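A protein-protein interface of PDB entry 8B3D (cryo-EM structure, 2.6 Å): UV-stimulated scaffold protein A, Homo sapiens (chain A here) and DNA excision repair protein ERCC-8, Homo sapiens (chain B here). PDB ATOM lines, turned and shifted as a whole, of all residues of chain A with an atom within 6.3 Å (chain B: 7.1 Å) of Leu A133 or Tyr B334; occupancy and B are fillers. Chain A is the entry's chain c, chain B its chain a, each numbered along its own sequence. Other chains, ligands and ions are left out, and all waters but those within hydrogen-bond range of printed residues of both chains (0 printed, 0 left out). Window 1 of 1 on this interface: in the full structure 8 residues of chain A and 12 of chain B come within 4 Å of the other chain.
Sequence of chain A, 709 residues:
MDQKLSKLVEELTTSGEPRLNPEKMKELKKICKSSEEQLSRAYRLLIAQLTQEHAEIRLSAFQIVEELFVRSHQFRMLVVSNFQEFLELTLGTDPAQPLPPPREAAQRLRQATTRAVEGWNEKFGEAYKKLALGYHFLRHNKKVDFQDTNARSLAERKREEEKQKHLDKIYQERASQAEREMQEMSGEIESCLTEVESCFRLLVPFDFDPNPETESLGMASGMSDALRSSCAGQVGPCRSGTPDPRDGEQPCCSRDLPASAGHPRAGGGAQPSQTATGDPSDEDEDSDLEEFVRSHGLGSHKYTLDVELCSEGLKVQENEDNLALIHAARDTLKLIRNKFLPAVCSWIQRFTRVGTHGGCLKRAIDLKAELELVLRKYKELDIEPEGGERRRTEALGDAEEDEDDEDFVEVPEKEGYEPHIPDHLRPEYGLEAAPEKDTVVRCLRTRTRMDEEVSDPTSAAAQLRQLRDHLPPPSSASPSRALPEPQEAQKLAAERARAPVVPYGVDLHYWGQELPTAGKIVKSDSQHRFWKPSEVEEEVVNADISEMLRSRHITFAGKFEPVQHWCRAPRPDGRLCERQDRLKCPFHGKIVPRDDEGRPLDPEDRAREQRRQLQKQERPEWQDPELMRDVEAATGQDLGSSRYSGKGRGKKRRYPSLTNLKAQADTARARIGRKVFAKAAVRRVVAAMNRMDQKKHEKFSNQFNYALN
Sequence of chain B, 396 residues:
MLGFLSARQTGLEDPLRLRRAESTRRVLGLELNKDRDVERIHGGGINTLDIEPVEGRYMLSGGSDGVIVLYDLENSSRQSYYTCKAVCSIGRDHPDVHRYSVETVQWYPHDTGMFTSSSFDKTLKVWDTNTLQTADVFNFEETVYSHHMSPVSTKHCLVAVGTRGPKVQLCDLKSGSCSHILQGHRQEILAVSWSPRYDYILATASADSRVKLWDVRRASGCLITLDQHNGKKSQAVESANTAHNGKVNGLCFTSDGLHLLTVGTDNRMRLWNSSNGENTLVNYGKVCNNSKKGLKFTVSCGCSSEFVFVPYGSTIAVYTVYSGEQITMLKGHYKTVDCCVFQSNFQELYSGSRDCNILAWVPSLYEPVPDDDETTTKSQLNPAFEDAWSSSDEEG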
ATOM      1  N   PHE A  83      -8.801  10.602  -0.546  1.00  0.00           N
ATOM      2  CA  PHE A  83      -9.793  11.672  -0.498  1.00  0.00           C
ATOM      3  C   PHE A  83     -10.692  11.701  -1.727  1.00  0.00           C
ATOM      4  O   PHE A  83     -11.836  12.152  -1.634  1.00  0.00           O
ATOM      5  CB  PHE A  83      -9.104  13.025  -0.337  1.00  0.00           C
ATOM      6  CG  PHE A  83      -9.931  14.036   0.401  1.00  0.00           C
ATOM      7  CD1 PHE A  83      -9.922  14.083   1.784  1.00  0.00           C
ATOM      8  CD2 PHE A  83     -10.701  14.954  -0.290  1.00  0.00           C
ATOM      9  CE1 PHE A  83     -10.685  15.013   2.464  1.00  0.00           C
ATOM     10  CE2 PHE A  83     -11.460  15.890   0.385  1.00  0.00           C
ATOM     11  CZ  PHE A  83     -11.449  15.921   1.762  1.00  0.00           C
ATOM     12  N   GLN A  84     -10.207  11.254  -2.888  1.00  0.00           N
ATOM     13  CA  GLN A  84     -11.071  11.222  -4.066  1.00  0.00           C
ATOM     14  C   GLN A  84     -12.273  10.314  -3.827  1.00  0.00           C
ATOM     15  O   GLN A  84     -13.427  10.728  -4.005  1.00  0.00           O
ATOM     16  CB  GLN A  84     -10.279  10.761  -5.290  1.00  0.00           C
ATOM     17  CG  GLN A  84     -11.076  10.783  -6.591  1.00  0.00           C
ATOM     18  CD  GLN A  84     -10.247  10.376  -7.794  1.00  0.00           C
ATOM     19  OE1 GLN A  84      -9.071  10.038  -7.666  1.00  0.00           O
ATOM     20  NE2 GLN A  84     -10.857  10.414  -8.973  1.00  0.00           N
ATOM     21  N   LEU A  87     -14.622  11.795  -1.182  1.00  0.00           N
ATOM     22  CA  LEU A  87     -15.560  12.773  -1.722  1.00  0.00           C
ATOM     23  C   LEU A  87     -16.632  12.114  -2.577  1.00  0.00           C
ATOM     24  O   LEU A  87     -17.789  12.542  -2.543  1.00  0.00           O
ATOM     25  CB  LEU A  87     -14.825  13.832  -2.540  1.00  0.00           C
ATOM     26  CG  LEU A  87     -13.878  14.749  -1.768  1.00  0.00           C
ATOM     27  CD1 LEU A  87     -13.124  15.649  -2.734  1.00  0.00           C
ATOM     28  CD2 LEU A  87     -14.649  15.573  -0.744  1.00  0.00           C
ATOM     29  N   GLU A  88     -16.275  11.085  -3.347  1.00  0.00           N
ATOM     30  CA  GLU A  88     -17.286  10.404  -4.150  1.00  0.00           C
ATOM     31  C   GLU A  88     -18.361   9.788  -3.265  1.00  0.00           C
ATOM     32  O   GLU A  88     -19.551   9.825  -3.599  1.00  0.00           O
ATOM     33  CB  GLU A  88     -16.639   9.332  -5.031  1.00  0.00           C
ATOM     34  CG  GLU A  88     -15.761   9.870  -6.158  1.00  0.00           C
ATOM     35  CD  GLU A  88     -16.520  10.768  -7.112  1.00  0.00           C
ATOM     36  OE1 GLU A  88     -17.756  10.623  -7.199  1.00  0.00           O
ATOM     37  OE2 GLU A  88     -15.884  11.617  -7.770  1.00  0.00           O
ATOM     38  N   TYR A 128      -1.664  19.460   4.068  1.00  0.00           N
ATOM     39  CA  TYR A 128      -2.120  18.453   3.111  1.00  0.00           C
ATOM     40  C   TYR A 128      -2.615  19.196   1.873  1.00  0.00           C
ATOM     41  O   TYR A 128      -3.783  19.585   1.802  1.00  0.00           O
ATOM     42  CB  TYR A 128      -3.217  17.594   3.712  1.00  0.00           C
ATOM     43  CG  TYR A 128      -2.859  16.902   5.004  1.00  0.00           C
ATOM     44  CD1 TYR A 128      -2.209  15.679   5.004  1.00  0.00           C
ATOM     45  CD2 TYR A 128      -3.188  17.470   6.225  1.00  0.00           C
ATOM     46  CE1 TYR A 128      -1.890  15.045   6.187  1.00  0.00           C
ATOM     47  CE2 TYR A 128      -2.873  16.844   7.412  1.00  0.00           C
ATOM     48  CZ  TYR A 128      -2.225  15.631   7.388  1.00  0.00           C
ATOM     49  OH  TYR A 128      -1.910  15.005   8.570  1.00  0.00           O
ATOM     50  N   LYS A 129      -1.728  19.396   0.896  1.00  0.00           N
ATOM     51  CA  LYS A 129      -2.115  20.133  -0.302  1.00  0.00           C
ATOM     52  C   LYS A 129      -3.137  19.366  -1.135  1.00  0.00           C
ATOM     53  O   LYS A 129      -3.852  19.970  -1.942  1.00  0.00           O
ATOM     54  CB  LYS A 129      -0.878  20.456  -1.143  1.00  0.00           C
ATOM     55  CG  LYS A 129       0.175  21.360  -0.468  1.00  0.00           C
ATOM     56  CD  LYS A 129      -0.392  22.589   0.256  1.00  0.00           C
ATOM     57  CE  LYS A 129      -1.050  23.581  -0.696  1.00  0.00           C
ATOM     58  NZ  LYS A 129      -2.008  24.471   0.015  1.00  0.00           N
ATOM     59  N   LYS A 130      -3.222  18.044  -0.970  1.00  0.00           N
ATOM     60  CA  LYS A 130      -4.257  17.291  -1.672  1.00  0.00           C
ATOM     61  C   LYS A 130      -5.642  17.627  -1.129  1.00  0.00           C
ATOM     62  O   LYS A 130      -6.625  17.640  -1.879  1.00  0.00           O
ATOM     63  CB  LYS A 130      -3.974  15.794  -1.572  1.00  0.00           C
ATOM     64  CG  LYS A 130      -5.032  14.912  -2.222  1.00  0.00           C
ATOM     65  CD  LYS A 130      -4.542  13.480  -2.400  1.00  0.00           C
ATOM     66  CE  LYS A 130      -4.187  13.179  -3.849  1.00  0.00           C
ATOM     67  NZ  LYS A 130      -3.306  11.985  -3.969  1.00  0.00           N
ATOM     68  N   LEU A 131      -5.741  17.909   0.173  1.00  0.00           N
ATOM     69  CA  LEU A 131      -6.980  18.462   0.711  1.00  0.00           C
ATOM     70  C   LEU A 131      -7.304  19.804   0.073  1.00  0.00           C
ATOM     71  O   LEU A 131      -8.472  20.101  -0.201  1.00  0.00           O
ATOM     72  CB  LEU A 131      -6.882  18.608   2.230  1.00  0.00           C
ATOM     73  CG  LEU A 131      -6.678  17.358   3.087  1.00  0.00           C
ATOM     74  CD1 LEU A 131      -7.060  17.662   4.516  1.00  0.00           C
ATOM     75  CD2 LEU A 131      -7.520  16.216   2.582  1.00  0.00           C
ATOM     76  N   ALA A 132      -6.289  20.638  -0.156  1.00  0.00           N
ATOM     77  CA  ALA A 132      -6.528  21.901  -0.847  1.00  0.00           C
ATOM     78  C   ALA A 132      -7.038  21.657  -2.260  1.00  0.00           C
ATOM     79  O   ALA A 132      -7.945  22.354  -2.730  1.00  0.00           O
ATOM     80  CB  ALA A 132      -5.250  22.738  -0.871  1.00  0.00           C
ATOM     81  N   LEU A 133      -6.470  20.667  -2.953  1.00  0.00           N
ATOM     82  CA  LEU A 133      -6.938  20.331  -4.293  1.00  0.00           C
ATOM     83  C   LEU A 133      -8.393  19.881  -4.265  1.00  0.00           C
ATOM     84  O   LEU A 133      -9.202  20.302  -5.099  1.00  0.00           O
ATOM     85  CB  LEU A 133      -6.057  19.238  -4.900  1.00  0.00           C
ATOM     86  CG  LEU A 133      -4.613  19.605  -5.247  1.00  0.00           C
ATOM     87  CD1 LEU A 133      -3.857  18.366  -5.694  1.00  0.00           C
ATOM     88  CD2 LEU A 133      -4.564  20.675  -6.325  1.00  0.00           C
ATOM     89  N   GLY A 134      -8.741  19.024  -3.305  1.00  0.00           N
ATOM     90  CA  GLY A 134     -10.120  18.573  -3.196  1.00  0.00           C
ATOM     91  C   GLY A 134     -11.080  19.705  -2.882  1.00  0.00           C
ATOM     92  O   GLY A 134     -12.161  19.796  -3.469  1.00  0.00           O
ATOM     93  N   TYR A 135     -10.696  20.583  -1.954  1.00  0.00           N
ATOM     94  CA  TYR A 135     -11.535  21.728  -1.616  1.00  0.00           C
ATOM     95  C   TYR A 135     -11.741  22.634  -2.822  1.00  0.00           C
ATOM     96  O   TYR A 135     -12.862  23.076  -3.096  1.00  0.00           O
ATOM     97  CB  TYR A 135     -10.904  22.508  -0.463  1.00  0.00           C
ATOM     98  CG  TYR A 135     -11.766  23.628   0.065  1.00  0.00           C
ATOM     99  CD1 TYR A 135     -12.730  23.388   1.030  1.00  0.00           C
ATOM    100  CD2 TYR A 135     -11.613  24.926  -0.398  1.00  0.00           C
ATOM    101  CE1 TYR A 135     -13.522  24.406   1.518  1.00  0.00           C
ATOM    102  CE2 TYR A 135     -12.398  25.952   0.085  1.00  0.00           C
ATOM    103  CZ  TYR A 135     -13.352  25.688   1.041  1.00  0.00           C
ATOM    104  OH  TYR A 135     -14.136  26.711   1.517  1.00  0.00           O
ATOM    105  N   HIS A 136     -10.665  22.918  -3.558  1.00  0.00           N
ATOM    106  CA  HIS A 136     -10.768  23.763  -4.740  1.00  0.00           C
ATOM    107  C   HIS A 136     -11.658  23.118  -5.796  1.00  0.00           C
ATOM    108  O   HIS A 136     -12.498  23.789  -6.413  1.00  0.00           O
ATOM    109  CB  HIS A 136      -9.366  24.021  -5.290  1.00  0.00           C
ATOM    110  CG  HIS A 136      -9.301  25.114  -6.306  1.00  0.00           C
ATOM    111  ND1 HIS A 136      -9.044  26.425  -5.969  1.00  0.00           N
ATOM    112  CD2 HIS A 136      -9.440  25.091  -7.651  1.00  0.00           C
ATOM    113  CE1 HIS A 136      -9.036  27.164  -7.064  1.00  0.00           C
ATOM    114  NE2 HIS A 136      -9.274  26.378  -8.098  1.00  0.00           N
ATOM    115  N   PHE A 137     -11.492  21.810  -6.002  1.00  0.00           N
ATOM    116  CA  PHE A 137     -12.294  21.089  -6.982  1.00  0.00           C
ATOM    117  C   PHE A 137     -13.770  21.134  -6.611  1.00  0.00           C
ATOM    118  O   PHE A 137     -14.633  21.345  -7.471  1.00  0.00           O
ATOM    119  CB  PHE A 137     -11.792  19.648  -7.075  1.00  0.00           C
ATOM    120  CG  PHE A 137     -12.669  18.744  -7.887  1.00  0.00           C
ATOM    121  CD1 PHE A 137     -12.561  18.713  -9.266  1.00  0.00           C
ATOM    122  CD2 PHE A 137     -13.588  17.912  -7.272  1.00  0.00           C
ATOM    123  CE1 PHE A 137     -13.359  17.878 -10.016  1.00  0.00           C
ATOM    124  CE2 PHE A 137     -14.390  17.074  -8.018  1.00  0.00           C
ATOM    125  CZ  PHE A 137     -14.274  17.057  -9.391  1.00  0.00           C
ATOM    126  N   LEU A 138     -14.081  20.942  -5.328  1.00  0.00           N
ATOM    127  CA  LEU A 138     -15.466  21.053  -4.886  1.00  0.00           C
ATOM    128  C   LEU A 138     -15.997  22.466  -5.091  1.00  0.00           C
ATOM    129  O   LEU A 138     -17.142  22.650  -5.521  1.00  0.00           O
ATOM    130  CB  LEU A 138     -15.589  20.655  -3.414  1.00  0.00           C
ATOM    131  CG  LEU A 138     -15.378  19.194  -3.002  1.00  0.00           C
ATOM    132  CD1 LEU A 138     -15.816  19.010  -1.559  1.00  0.00           C
ATOM    133  CD2 LEU A 138     -16.123  18.226  -3.907  1.00  0.00           C
ATOM    134  N   LEU B  32       3.542  12.525  -5.305  1.00  0.00           N
ATOM    135  CA  LEU B  32       2.904  13.836  -5.322  1.00  0.00           C
ATOM    136  C   LEU B  32       3.885  14.807  -4.655  1.00  0.00           C
ATOM    137  O   LEU B  32       4.418  14.516  -3.580  1.00  0.00           O
ATOM    138  CB  LEU B  32       1.581  13.788  -4.554  1.00  0.00           C
ATOM    139  CG  LEU B  32       0.568  14.904  -4.817  1.00  0.00           C
ATOM    140  CD1 LEU B  32       0.834  16.117  -3.938  1.00  0.00           C
ATOM    141  CD2 LEU B  32       0.573  15.294  -6.288  1.00  0.00           C
ATOM    142  N   ASN B  33       4.091  15.980  -5.249  1.00  0.00           N
ATOM    143  CA  ASN B  33       5.084  16.905  -4.717  1.00  0.00           C
ATOM    144  C   ASN B  33       4.782  17.395  -3.291  1.00  0.00           C
ATOM    145  O   ASN B  33       3.707  17.934  -3.034  1.00  0.00           O
ATOM    146  CB  ASN B  33       5.181  18.117  -5.646  1.00  0.00           C
ATOM    147  CG  ASN B  33       3.823  18.681  -6.020  1.00  0.00           C
ATOM    148  OD1 ASN B  33       2.815  18.376  -5.385  1.00  0.00           O
ATOM    149  ND2 ASN B  33       3.792  19.506  -7.060  1.00  0.00           N
ATOM    150  N   ASP B  37       4.090  23.684  -5.933  1.00  0.00           N
ATOM    151  CA  ASP B  37       2.747  23.988  -6.413  1.00  0.00           C
ATOM    152  C   ASP B  37       2.823  24.698  -7.760  1.00  0.00           C
ATOM    153  O   ASP B  37       3.825  25.338  -8.073  1.00  0.00           O
ATOM    154  CB  ASP B  37       1.999  24.860  -5.403  1.00  0.00           C
ATOM    155  CG  ASP B  37       1.338  24.047  -4.306  1.00  0.00           C
ATOM    156  OD1 ASP B  37       0.774  22.977  -4.615  1.00  0.00           O
ATOM    157  OD2 ASP B  37       1.372  24.486  -3.137  1.00  0.00           O
ATOM    158  N   ARG B  40      -2.683  28.263 -10.662  1.00  0.00           N
ATOM    159  CA  ARG B  40      -3.882  27.881 -11.397  1.00  0.00           C
ATOM    160  C   ARG B  40      -4.457  29.092 -12.122  1.00  0.00           C
ATOM    161  O   ARG B  40      -4.880  30.058 -11.479  1.00  0.00           O
ATOM    162  CB  ARG B  40      -4.917  27.300 -10.442  1.00  0.00           C
ATOM    163  CG  ARG B  40      -5.917  26.382 -11.105  1.00  0.00           C
ATOM    164  CD  ARG B  40      -6.934  25.870 -10.109  1.00  0.00           C
ATOM    165  NE  ARG B  40      -6.427  24.767  -9.294  1.00  0.00           N
ATOM    166  CZ  ARG B  40      -5.831  24.904  -8.112  1.00  0.00           C
ATOM    167  NH1 ARG B  40      -5.657  26.102  -7.569  1.00  0.00           N
ATOM    168  NH2 ARG B  40      -5.410  23.829  -7.462  1.00  0.00           N
ATOM    169  N   SER B 314      -7.885   8.861 -14.448  1.00  0.00           N
ATOM    170  CA  SER B 314      -7.467  10.017 -13.670  1.00  0.00           C
ATOM    171  C   SER B 314      -6.093   9.827 -13.041  1.00  0.00           C
ATOM    172  O   SER B 314      -5.802  10.445 -12.011  1.00  0.00           O
ATOM    173  CB  SER B 314      -8.500  10.317 -12.584  1.00  0.00           C
ATOM    174  OG  SER B 314      -8.581   9.251 -11.654  1.00  0.00           O
ATOM    175  N   GLY B 332      -3.192  11.481  -8.286  1.00  0.00           N
ATOM    176  CA  GLY B 332      -3.502  12.733  -7.624  1.00  0.00           C
ATOM    177  C   GLY B 332      -4.498  13.623  -8.339  1.00  0.00           C
ATOM    178  O   GLY B 332      -4.840  14.694  -7.830  1.00  0.00           O
ATOM    179  N   HIS B 333      -4.983  13.199  -9.499  1.00  0.00           N
ATOM    180  CA  HIS B 333      -5.925  13.994 -10.269  1.00  0.00           C
ATOM    181  C   HIS B 333      -7.355  13.569  -9.967  1.00  0.00           C
ATOM    182  O   HIS B 333      -7.625  12.424  -9.597  1.00  0.00           O
ATOM    183  CB  HIS B 333      -5.646  13.872 -11.766  1.00  0.00           C
ATOM    184  CG  HIS B 333      -4.583  14.803 -12.254  1.00  0.00           C
ATOM    185  ND1 HIS B 333      -4.800  16.152 -12.419  1.00  0.00           N
ATOM    186  CD2 HIS B 333      -3.299  14.581 -12.616  1.00  0.00           C
ATOM    187  CE1 HIS B 333      -3.695  16.724 -12.860  1.00  0.00           C
ATOM    188  NE2 HIS B 333      -2.769  15.793 -12.989  1.00  0.00           N
ATOM    189  N   TYR B 334      -8.277  14.515 -10.136  1.00  0.00           N
ATOM    190  CA  TYR B 334      -9.682  14.299  -9.827  1.00  0.00           C
ATOM    191  C   TYR B 334     -10.532  13.985 -11.045  1.00  0.00           C
ATOM    192  O   TYR B 334     -11.632  13.455 -10.888  1.00  0.00           O
ATOM    193  CB  TYR B 334     -10.259  15.528  -9.118  1.00  0.00           C
ATOM    194  CG  TYR B 334      -9.826  15.626  -7.676  1.00  0.00           C
ATOM    195  CD1 TYR B 334     -10.323  14.748  -6.724  1.00  0.00           C
ATOM    196  CD2 TYR B 334      -8.910  16.582  -7.270  1.00  0.00           C
ATOM    197  CE1 TYR B 334      -9.927  14.827  -5.406  1.00  0.00           C
ATOM    198  CE2 TYR B 334      -8.507  16.669  -5.954  1.00  0.00           C
ATOM    199  CZ  TYR B 334      -9.018  15.789  -5.026  1.00  0.00           C
ATOM    200  OH  TYR B 334      -8.620  15.871  -3.712  1.00  0.00           O
ATOM    201  N   LYS B 335     -10.056  14.299 -12.242  1.00  0.00           N
ATOM    202  CA  LYS B 335     -10.711  13.933 -13.488  1.00  0.00           C
ATOM    203  C   LYS B 335      -9.685  13.308 -14.427  1.00  0.00           C
ATOM    204  O   LYS B 335      -8.506  13.177 -14.093  1.00  0.00           O
ATOM    205  CB  LYS B 335     -11.385  15.148 -14.129  1.00  0.00           C
ATOM    206  N   THR B 336     -10.152  12.908 -15.607  1.00  0.00           N
ATOM    207  CA  THR B 336      -9.284  12.231 -16.559  1.00  0.00           C
ATOM    208  C   THR B 336      -8.103  13.120 -16.925  1.00  0.00           C
ATOM    209  O   THR B 336      -8.247  14.325 -17.142  1.00  0.00           O
ATOM    210  CB  THR B 336     -10.058  11.852 -17.822  1.00  0.00           C
ATOM    211  OG1 THR B 336     -10.556  13.038 -18.456  1.00  0.00           O
ATOM    212  CG2 THR B 336     -11.220  10.925 -17.489  1.00  0.00           C
ATOM    213  N   VAL B 337      -6.920  12.519 -16.969  1.00  0.00           N
ATOM    214  CA  VAL B 337      -5.689  13.238 -17.270  1.00  0.00           C
ATOM    215  C   VAL B 337      -5.552  13.339 -18.780  1.00  0.00           C
ATOM    216  O   VAL B 337      -5.641  12.330 -19.490  1.00  0.00           O
ATOM    217  CB  VAL B 337      -4.464  12.545 -16.651  1.00  0.00           C
ATOM    218  CG1 VAL B 337      -3.198  13.313 -17.002  1.00  0.00           C
ATOM    219  CG2 VAL B 337      -4.624  12.428 -15.146  1.00  0.00           C
ATOM    220  N   SER B 353      -4.940  17.912 -16.491  1.00  0.00           N
ATOM    221  CA  SER B 353      -6.149  17.104 -16.499  1.00  0.00           C
ATOM    222  C   SER B 353      -7.364  18.009 -16.639  1.00  0.00           C
ATOM    223  O   SER B 353      -7.252  19.236 -16.681  1.00  0.00           O
ATOM    224  CB  SER B 353      -6.248  16.261 -15.227  1.00  0.00           C
ATOM    225  OG  SER B 353      -7.338  15.364 -15.294  1.00  0.00           O
ATOM    226  N   ARG B 354      -8.538  17.379 -16.710  1.00  0.00           N
ATOM    227  CA  ARG B 354      -9.786  18.111 -16.886  1.00  0.00           C
ATOM    228  C   ARG B 354     -10.211  18.879 -15.642  1.00  0.00           C
ATOM    229  O   ARG B 354     -11.151  19.675 -15.727  1.00  0.00           O
ATOM    230  CB  ARG B 354     -10.912  17.152 -17.288  1.00  0.00           C
ATOM    231  CG  ARG B 354     -10.637  16.274 -18.510  1.00  0.00           C
ATOM    232  CD  ARG B 354      -9.929  17.005 -19.642  1.00  0.00           C
ATOM    233  NE  ARG B 354     -10.647  18.212 -20.048  1.00  0.00           N
ATOM    234  CZ  ARG B 354     -10.694  18.701 -21.286  1.00  0.00           C
ATOM    235  NH1 ARG B 354     -10.049  18.117 -22.290  1.00  0.00           N
ATOM    236  NH2 ARG B 354     -11.389  19.803 -21.520  1.00  0.00           N
ATOM    237  N   ASP B 355      -9.558  18.669 -14.499  1.00  0.00           N
ATOM    238  CA  ASP B 355      -9.932  19.348 -13.265  1.00  0.00           C
ATOM    239  C   ASP B 355      -9.298  20.727 -13.131  1.00  0.00           C
ATOM    240  O   ASP B 355      -9.256  21.264 -12.018  1.00  0.00           O
ATOM    241  CB  ASP B 355      -9.551  18.491 -12.057  1.00  0.00           C
ATOM    242  CG  ASP B 355      -8.058  18.322 -11.914  1.00  0.00           C
ATOM    243  OD1 ASP B 355      -7.360  18.388 -12.942  1.00  0.00           O
ATOM    244  OD2 ASP B 355      -7.581  18.126 -10.778  1.00  0.00           O
ATOM    245  N   ASN B 357      -6.230  21.639 -13.207  1.00  0.00           N
ATOM    246  CA  ASN B 357      -5.042  21.574 -12.368  1.00  0.00           C
ATOM    247  C   ASN B 357      -3.863  21.060 -13.178  1.00  0.00           C
ATOM    248  O   ASN B 357      -4.007  20.174 -14.023  1.00  0.00           O
ATOM    249  CB  ASN B 357      -5.249  20.655 -11.160  1.00  0.00           C
ATOM    250  CG  ASN B 357      -6.038  21.314 -10.057  1.00  0.00           C
ATOM    251  OD1 ASN B 357      -5.822  22.481  -9.742  1.00  0.00           O
ATOM    252  ND2 ASN B 357      -6.954  20.566  -9.455  1.00  0.00           N
ATOM    253  N   ILE B 358      -2.693  21.631 -12.908  1.00  0.00           N
ATOM    254  CA  ILE B 358      -1.420  21.095 -13.370  1.00  0.00           C
ATOM    255  C   ILE B 358      -0.676  20.623 -12.132  1.00  0.00           C
ATOM    256  O   ILE B 358      -0.273  21.439 -11.295  1.00  0.00           O
ATOM    257  CB  ILE B 358      -0.591  22.126 -14.154  1.00  0.00           C
ATOM    258  CG1 ILE B 358      -1.433  22.773 -15.261  1.00  0.00           C
ATOM    259  CG2 ILE B 358       0.645  21.458 -14.759  1.00  0.00           C
ATOM    260  CD1 ILE B 358      -0.738  23.905 -15.981  1.00  0.00           C
ATOM    261  N   LEU B 359      -0.496  19.312 -12.017  1.00  0.00           N
ATOM    262  CA  LEU B 359       0.123  18.707 -10.848  1.00  0.00           C
ATOM    263  C   LEU B 359       1.562  18.337 -11.166  1.00  0.00           C
ATOM    264  O   LEU B 359       1.847  17.782 -12.232  1.00  0.00           O
ATOM    265  CB  LEU B 359      -0.653  17.469 -10.398  1.00  0.00           C
ATOM    266  CG  LEU B 359      -2.072  17.694  -9.869  1.00  0.00           C
ATOM    267  CD1 LEU B 359      -2.651  16.387  -9.371  1.00  0.00           C
ATOM    268  CD2 LEU B 359      -2.104  18.739  -8.767  1.00  0.00           C
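N of Gly A134 sits close to OH of Tyr B334, 3.2 Å away.
The backbone carbonyl oxygen (O) of His B333 sits close to the side-chain amide oxygen (OE1) of Gln A84, at 3.4 Å.
OH of Tyr B334 lies within hydrogen-bond range of O of Lys A130, at 3.2 Å.
NE of Arg B40 sits close to NE2 of His A136 (3.5 Å).
The side-chain amide nitrogen (ND2) of Asn B357 lies within hydrogen-bond range of the side-chain carboxylate (OD2) of Asp B355, 2.8 Å away.
The guanidinium group (NE) of Arg B40 is in hydrogen-bond range of the side-chain amide oxygen (OD1) of Asn B357 (2.4 Å).
A ring nitrogen (ND1) of His B333 sits at hydrogen-bond distance from the side-chain carboxylate (OD1) of Asp B355.
OG of Ser B314 touches NE2 of Gln A84, at 3.7 Å.
NE2 of Gln A84 touches O of Tyr B334, 3.7 Å away.
Lys A129 touches Asp B37 (CE to OD2, 3.6 Å).
Lys A130 touches Gly B332.
CD2 of Leu A133 touches NH2 of Arg B40, 3.5 Å away.
Leu A133 touches Tyr B334 (C to CE2, 3.6 Å).
Asn B357 touches Leu A133 (ND2 to CD2, 3.9 Å).
Leu A133 touches Leu B359 (CD1 to CD2, 3.6 Å).
Phe A137 touches Tyr B334.
Of chain B, only Arg B40 (3.5 Å), Tyr B334 (3.6 Å), Asn B357 (3.9 Å) and Leu B359 (3.6 Å) come within 4 Å of Leu A133.
Of chain A, only Gln A84 (3.7 Å), Lys A130 (3.2 Å), Leu A133 (3.6 Å), Gly A134 (3.1 Å) and Phe A137 (3.9 Å) come within 4 Å of Tyr B334.
Of the printed residues of chain A, Asp B37 touches Lys A129 (3.6 Å).
Of the printed residues of chain A, Ser B314 touches Gln A84 (3.7 Å).
Printed residues of chain A within 4 Å of Asn B357: Leu A133 (3.9 Å).
Of the printed residues of chain B, Lys A129 touches Asp B37.
Ile B358 touches none of the printed residues of chain A.
Leu B32 touches none of the printed residues of chain A.
The nearest residue of chain A that does not touch Tyr B334 is Phe A83 (4.1 Å).
The nearest printed residue of chain A that does not touch His B333 is Lys A130 (5.7 Å).
Printed residues of chain A that touch a printed residue of chain B: Gln A84, Lys A129, Lys A130, Leu A133, Gly A134, His A136 and Phe A137.
Hydrophobic or aromatic side chains of chain A within 4 Å of the printed part of chain B: Leu A133, His A136 and Phe A137.
Along chain A the printed residues that touch a printed residue of chain B span positions 84 to 137.
Printed residues of chain B that touch a printed residue of chain A: Asp B37, Arg B40, Ser B314, Gly B332, His B333, Tyr B334, Asn B357 and Leu B359.
Hydrophobic or aromatic side chains of chain B within 4 Å of the printed part of chain A: Tyr B334 and Leu B359.
Among the printed residues, 13 pairs touch across the chains.
Among the printed residues, no Asp or Glu carboxylate lies within 4 Å of a Lys or Arg side-chain nitrogen of the other chain.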
